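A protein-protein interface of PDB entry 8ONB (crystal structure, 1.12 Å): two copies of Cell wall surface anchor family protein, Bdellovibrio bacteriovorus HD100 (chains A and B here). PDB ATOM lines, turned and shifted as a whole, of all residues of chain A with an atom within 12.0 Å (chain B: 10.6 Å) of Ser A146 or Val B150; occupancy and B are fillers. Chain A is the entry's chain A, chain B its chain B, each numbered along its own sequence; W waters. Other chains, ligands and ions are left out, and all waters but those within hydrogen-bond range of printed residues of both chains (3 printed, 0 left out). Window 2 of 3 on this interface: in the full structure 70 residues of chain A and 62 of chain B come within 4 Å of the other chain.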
ATOM      1  N   GLY A 138      -2.379  41.821  -6.559  1.00  0.00           N
ATOM      2  CA  GLY A 138      -1.764  41.182  -7.704  1.00  0.00           C
ATOM      3  C   GLY A 138      -2.094  39.697  -7.741  1.00  0.00           C
ATOM      4  O   GLY A 138      -3.174  39.274  -7.308  1.00  0.00           O
ATOM      5  N   THR A 139      -1.147  38.918  -8.241  1.00  0.00           N
ATOM      6  CA  THR A 139      -1.338  37.494  -8.490  1.00  0.00           C
ATOM      7  C   THR A 139      -0.814  36.655  -7.326  1.00  0.00           C
ATOM      8  O   THR A 139      -0.026  37.117  -6.484  1.00  0.00           O
ATOM      9  CB  THR A 139      -0.626  37.100  -9.777  1.00  0.00           C
ATOM     10  OG1 THR A 139       0.771  37.400  -9.625  1.00  0.00           O
ATOM     11  CG2 THR A 139      -1.202  37.860 -10.970  1.00  0.00           C
ATOM     12  N   ALA A 140      -1.189  35.383  -7.324  1.00  0.00           N
ATOM     13  CA  ALA A 140      -0.815  34.465  -6.256  1.00  0.00           C
ATOM     14  C   ALA A 140      -0.558  33.102  -6.864  1.00  0.00           C
ATOM     15  O   ALA A 140      -1.417  32.587  -7.593  1.00  0.00           O
ATOM     16  CB  ALA A 140      -1.920  34.370  -5.204  1.00  0.00           C
ATOM     17  N   GLY A 141       0.597  32.524  -6.572  1.00  0.00           N
ATOM     18  CA  GLY A 141       0.969  31.234  -7.101  1.00  0.00           C
ATOM     19  C   GLY A 141       1.318  30.261  -6.002  1.00  0.00           C
ATOM     20  O   GLY A 141       2.038  30.626  -5.070  1.00  0.00           O
ATOM     21  N   LEU A 142       0.814  29.034  -6.104  1.00  0.00           N
ATOM     22  CA  LEU A 142       1.049  27.990  -5.121  1.00  0.00           C
ATOM     23  C   LEU A 142       1.416  26.728  -5.881  1.00  0.00           C
ATOM     24  O   LEU A 142       0.691  26.326  -6.795  1.00  0.00           O
ATOM     25  CB  LEU A 142      -0.230  27.762  -4.295  1.00  0.00           C
ATOM     26  CG  LEU A 142      -0.156  26.724  -3.174  1.00  0.00           C
ATOM     27  CD1 LEU A 142       0.906  27.084  -2.127  1.00  0.00           C
ATOM     28  CD2 LEU A 142      -1.540  26.570  -2.520  1.00  0.00           C
ATOM     29  N   SER A 143       2.516  26.090  -5.513  1.00  0.00           N
ATOM     30  CA  SER A 143       2.972  24.978  -6.340  1.00  0.00           C
ATOM     31  C   SER A 143       2.125  23.722  -6.171  1.00  0.00           C
ATOM     32  O   SER A 143       2.174  22.843  -7.042  1.00  0.00           O
ATOM     33  CB  SER A 143       4.430  24.641  -6.047  1.00  0.00           C
ATOM     34  OG  SER A 143       4.565  24.108  -4.745  1.00  0.00           O
ATOM     35  N   THR A 144       1.367  23.595  -5.079  1.00  0.00           N
ATOM     36  CA  THR A 144       0.682  22.347  -4.750  1.00  0.00           C
ATOM     37  C   THR A 144      -0.815  22.349  -5.045  1.00  0.00           C
ATOM     38  O   THR A 144      -1.440  21.297  -4.869  1.00  0.00           O
ATOM     39  CB  THR A 144       0.863  21.991  -3.266  1.00  0.00           C
ATOM     40  OG1 THR A 144       0.456  23.105  -2.458  1.00  0.00           O
ATOM     41  CG2 THR A 144       2.295  21.606  -2.959  1.00  0.00           C
ATOM     42  N   GLY A 145      -1.413  23.467  -5.450  1.00  0.00           N
ATOM     43  CA  GLY A 145      -2.846  23.474  -5.698  1.00  0.00           C
ATOM     44  C   GLY A 145      -3.382  24.888  -5.816  1.00  0.00           C
ATOM     45  O   GLY A 145      -2.620  25.858  -5.792  1.00  0.00           O
ATOM     46  N   SER A 146      -4.702  24.993  -5.924  1.00  0.00           N
ATOM     47  CA  SER A 146      -5.346  26.287  -6.103  1.00  0.00           C
ATOM     48  C   SER A 146      -6.035  26.802  -4.848  1.00  0.00           C
ATOM     49  O   SER A 146      -6.537  27.931  -4.858  1.00  0.00           O
ATOM     50  CB  SER A 146      -6.377  26.222  -7.242  1.00  0.00           C
ATOM     51  OG  SER A 146      -7.381  25.275  -6.938  1.00  0.00           O
ATOM     52  N   ALA A 147      -6.084  26.016  -3.781  1.00  0.00           N
ATOM     53  CA  ALA A 147      -6.777  26.408  -2.562  1.00  0.00           C
ATOM     54  C   ALA A 147      -5.832  26.386  -1.369  1.00  0.00           C
ATOM     55  O   ALA A 147      -4.824  25.676  -1.366  1.00  0.00           O
ATOM     56  CB  ALA A 147      -7.971  25.475  -2.283  1.00  0.00           C
ATOM     57  N   TRP A 148      -6.195  27.142  -0.338  1.00  0.00           N
ATOM     58  CA  TRP A 148      -5.605  26.920   0.973  1.00  0.00           C
ATOM     59  C   TRP A 148      -6.195  25.665   1.597  1.00  0.00           C
ATOM     60  O   TRP A 148      -7.375  25.343   1.401  1.00  0.00           O
ATOM     61  CB  TRP A 148      -5.949  28.062   1.920  1.00  0.00           C
ATOM     62  CG  TRP A 148      -5.579  29.457   1.524  1.00  0.00           C
ATOM     63  CD1 TRP A 148      -6.294  30.302   0.714  1.00  0.00           C
ATOM     64  CD2 TRP A 148      -4.480  30.230   2.037  1.00  0.00           C
ATOM     65  NE1 TRP A 148      -5.700  31.541   0.671  1.00  0.00           N
ATOM     66  CE2 TRP A 148      -4.578  31.522   1.471  1.00  0.00           C
ATOM     67  CE3 TRP A 148      -3.415  29.947   2.900  1.00  0.00           C
ATOM     68  CZ2 TRP A 148      -3.650  32.529   1.749  1.00  0.00           C
ATOM     69  CZ3 TRP A 148      -2.496  30.956   3.184  1.00  0.00           C
ATOM     70  CH2 TRP A 148      -2.633  32.232   2.613  1.00  0.00           C
ATOM     71  N   THR A 149      -5.372  24.954   2.363  1.00  0.00           N
ATOM     72  CA  THR A 149      -5.873  23.924   3.254  1.00  0.00           C
ATOM     73  C   THR A 149      -6.505  24.599   4.470  1.00  0.00           C
ATOM     74  O   THR A 149      -5.934  25.536   5.023  1.00  0.00           O
ATOM     75  CB  THR A 149      -4.728  23.005   3.680  1.00  0.00           C
ATOM     76  OG1 THR A 149      -4.181  22.362   2.520  1.00  0.00           O
ATOM     77  CG2 THR A 149      -5.203  21.942   4.670  1.00  0.00           C
ATOM     78  N   VAL A 150      -7.693  24.157   4.866  1.00  0.00           N
ATOM     79  CA  VAL A 150      -8.289  24.676   6.093  1.00  0.00           C
ATOM     80  C   VAL A 150      -7.463  24.172   7.270  1.00  0.00           C
ATOM     81  O   VAL A 150      -7.352  22.961   7.488  1.00  0.00           O
ATOM     82  CB  VAL A 150      -9.748  24.227   6.222  1.00  0.00           C
ATOM     83  CG1 VAL A 150     -10.341  24.802   7.490  1.00  0.00           C
ATOM     84  CG2 VAL A 150     -10.535  24.673   5.006  1.00  0.00           C
ATOM     85  N   LEU B 142      -7.047  38.813  -1.541  1.00  0.00           N
ATOM     86  CA  LEU B 142      -6.304  38.802  -2.801  1.00  0.00           C
ATOM     87  C   LEU B 142      -7.060  39.691  -3.784  1.00  0.00           C
ATOM     88  O   LEU B 142      -8.264  39.522  -3.964  1.00  0.00           O
ATOM     89  CB  LEU B 142      -6.185  37.353  -3.335  1.00  0.00           C
ATOM     90  CG  LEU B 142      -5.397  37.177  -4.626  1.00  0.00           C
ATOM     91  CD1 LEU B 142      -3.942  37.677  -4.468  1.00  0.00           C
ATOM     92  CD2 LEU B 142      -5.430  35.713  -5.083  1.00  0.00           C
ATOM     93  N   GLY B 145      -8.683  37.609  -7.211  1.00  0.00           N
ATOM     94  CA  GLY B 145      -9.570  36.458  -7.227  1.00  0.00           C
ATOM     95  C   GLY B 145      -9.541  35.740  -5.895  1.00  0.00           C
ATOM     96  O   GLY B 145      -8.912  36.199  -4.945  1.00  0.00           O
ATOM     97  N   SER B 146     -10.195  34.587  -5.856  1.00  0.00           N
ATOM     98  CA  SER B 146     -10.304  33.827  -4.620  1.00  0.00           C
ATOM     99  C   SER B 146      -9.407  32.601  -4.599  1.00  0.00           C
ATOM    100  O   SER B 146      -9.281  31.965  -3.545  1.00  0.00           O
ATOM    101  CB  SER B 146     -11.766  33.397  -4.393  1.00  0.00           C
ATOM    102  OG  SER B 146     -12.205  32.526  -5.431  1.00  0.00           O
ATOM    103  N   ALA B 147      -8.768  32.260  -5.715  1.00  0.00           N
ATOM    104  CA  ALA B 147      -7.968  31.050  -5.842  1.00  0.00           C
ATOM    105  C   ALA B 147      -6.499  31.406  -6.056  1.00  0.00           C
ATOM    106  O   ALA B 147      -6.167  32.471  -6.589  1.00  0.00           O
ATOM    107  CB  ALA B 147      -8.451  30.192  -7.022  1.00  0.00           C
ATOM    108  N   TRP B 148      -5.609  30.530  -5.596  1.00  0.00           N
ATOM    109  CA  TRP B 148      -4.232  30.615  -6.041  1.00  0.00           C
ATOM    110  C   TRP B 148      -4.139  30.060  -7.455  1.00  0.00           C
ATOM    111  O   TRP B 148      -4.879  29.144  -7.819  1.00  0.00           O
ATOM    112  CB  TRP B 148      -3.342  29.718  -5.187  1.00  0.00           C
ATOM    113  CG  TRP B 148      -3.266  29.931  -3.697  1.00  0.00           C
ATOM    114  CD1 TRP B 148      -4.153  29.481  -2.744  1.00  0.00           C
ATOM    115  CD2 TRP B 148      -2.182  30.533  -2.992  1.00  0.00           C
ATOM    116  NE1 TRP B 148      -3.689  29.787  -1.486  1.00  0.00           N
ATOM    117  CE2 TRP B 148      -2.482  30.436  -1.604  1.00  0.00           C
ATOM    118  CE3 TRP B 148      -0.982  31.132  -3.386  1.00  0.00           C
ATOM    119  CZ2 TRP B 148      -1.616  30.908  -0.625  1.00  0.00           C
ATOM    120  CZ3 TRP B 148      -0.131  31.601  -2.417  1.00  0.00           C
ATOM    121  CH2 TRP B 148      -0.455  31.489  -1.048  1.00  0.00           C
ATOM    122  N   THR B 149      -3.219  30.598  -8.252  1.00  0.00           N
ATOM    123  CA  THR B 149      -2.826  29.943  -9.499  1.00  0.00           C
ATOM    124  C   THR B 149      -1.879  28.790  -9.182  1.00  0.00           C
ATOM    125  O   THR B 149      -0.979  28.930  -8.354  1.00  0.00           O
ATOM    126  CB  THR B 149      -2.095  30.950 -10.391  1.00  0.00           C
ATOM    127  OG1 THR B 149      -2.939  32.085 -10.654  1.00  0.00           O
ATOM    128  CG2 THR B 149      -1.631  30.304 -11.701  1.00  0.00           C
ATOM    129  N   VAL B 150      -2.075  27.641  -9.825  1.00  0.00           N
ATOM    130  CA  VAL B 150      -1.160  26.531  -9.603  1.00  0.00           C
ATOM    131  C   VAL B 150       0.159  26.858 -10.293  1.00  0.00           C
ATOM    132  O   VAL B 150       0.204  27.032 -11.515  1.00  0.00           O
ATOM    133  CB  VAL B 150      -1.742  25.211 -10.119  1.00  0.00           C
ATOM    134  CG1 VAL B 150      -0.757  24.093  -9.822  1.00  0.00           C
ATOM    135  CG2 VAL B 150      -3.092  24.950  -9.473  1.00  0.00           C
ATOM    136  N   ALA B 151       1.226  26.962  -9.517  1.00  0.00           N
ATOM    137  CA  ALA B 151       2.538  27.381 -10.037  1.00  0.00           C
ATOM    138  C   ALA B 151       3.301  26.173 -10.554  1.00  0.00           C
ATOM    139  O   ALA B 151       3.349  25.154  -9.873  1.00  0.00           O
ATOM    140  CB  ALA B 151       3.352  28.098  -8.965  1.00  0.00           C
HETATM  141  O   HOH W   1      -3.039  34.556  -9.472  1.00  0.00           O
HETATM  142  O   HOH W   2       3.526  22.726  -9.351  1.00  0.00           O
HETATM  143  O   HOH W   3      -7.971  29.567  -2.692  1.00  0.00           O
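N of Thr B149 sits at hydrogen-bond distance from O of Ala A140 (2.8 Å). The backbone NH (N) of Leu A142 is in hydrogen-bond range of the backbone carbonyl oxygen (O) of Thr B149 (2.9 Å). The backbone NH (N) of Ala B151 lies within hydrogen-bond range of the backbone carbonyl oxygen (O) of Leu A142 (2.8 Å). N of Trp B148 sits at hydrogen-bond distance from O of Ser A146 (2.9 Å). NE1 of Trp A148 sits close to NE1 of Trp B148, 3.4 Å away.
Leu A142 touches Thr B149, but with the chains exchanged Thr A149 does not touch Leu B142 (13.1 Å). Leu A142 touches Val B150, but with the chains exchanged Val A150 does not touch Leu B142 (15.4 Å). Gly A145 touches Trp B148, but with the chains exchanged Trp A148 does not touch Gly B145 (8.0 Å). Trp B148 touches its own counterpart, Trp A148. 7 positions are printed for both chains.
Water W2 lies within hydrogen-bond range of the backbone carbonyl oxygen (O) of Ala B151 (2.5 Å) and the backbone carbonyl oxygen (O) of Ser A143 (2.7 Å). Water W1 bridges OG1 of Thr B149 (2.7 Å) and N of Ala A140 (3.0 Å). Water W3 lies within hydrogen-bond range of the backbone carbonyl oxygen (O) of Ser B146 (2.9 Å) and the backbone carbonyl oxygen (O) of Ser A146 (3.1 Å).
CD1 of Leu B142 touches O of Gly A138, at 3.3 Å. Leu B142 touches Ala A140 (CD2 to CB, 3.8 Å). Trp B148 touches Gly A141. O of Thr B149 touches CA of Gly A141 (3.3 Å). Leu A142 touches Trp B148. O of Leu A142 touches CA of Val B150, at 3.4 Å. CA of Ser A143 touches O of Ala B151 (3.6 Å). CB of Trp B148 touches O of Gly A145, at 3.97 Å. CG2 of Val B150 touches C of Gly A145, at 3.7 Å. Ser A146 touches Val B150 (N to CG2, 3.9 Å).
Printed residues of chain A that touch a printed residue of chain B: Gly A138, Ala A140, Gly A141, Leu A142, Ser A143, Gly A145, Ser A146, Ala A147 and Trp A148. Hydrophobic or aromatic side chains of chain A within 4 Å of the printed part of chain B: Ala A140, Leu A142 and Trp A148. Among the printed residues, 18 pairs touch across the chains.
Of chain B, only Ala B147, Trp B148 and Val B150 come within 4 Å of Ser A146. Of chain A, only Leu A142 (3.4 Å), Gly A145 (3.7 Å) and Ser A146 (3.9 Å) come within 4 Å of Val B150. Of chain B, only Trp B148 and Val B150 come within 4 Å of Gly A145. Of chain B, only Trp B148 (3.8 Å) comes within 4 Å of Ala A147. No residue of chain A comes within 4 Å of Ser B146. Ala B147 touches just one residue of chain A: Ser A146. Ala B151 touches just these residues of chain A: Leu A142 (2.8 Å) and Ser A143 (3.6 Å). Of the printed residues of chain B, Gly A138 touches Leu B142. Printed residues of chain A within 4 Å of Trp B148: Ala A140 (3.7 Å), Gly A141 (3.5 Å), Leu A142 (3.6 Å), Gly A145 (3.97 Å), Ser A146 (2.9 Å), Ala A147 (3.8 Å) and Trp A148 (3.4 Å). The nearest residue of chain B that does not touch Ser A146 is Ser B146 (5.1 Å).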
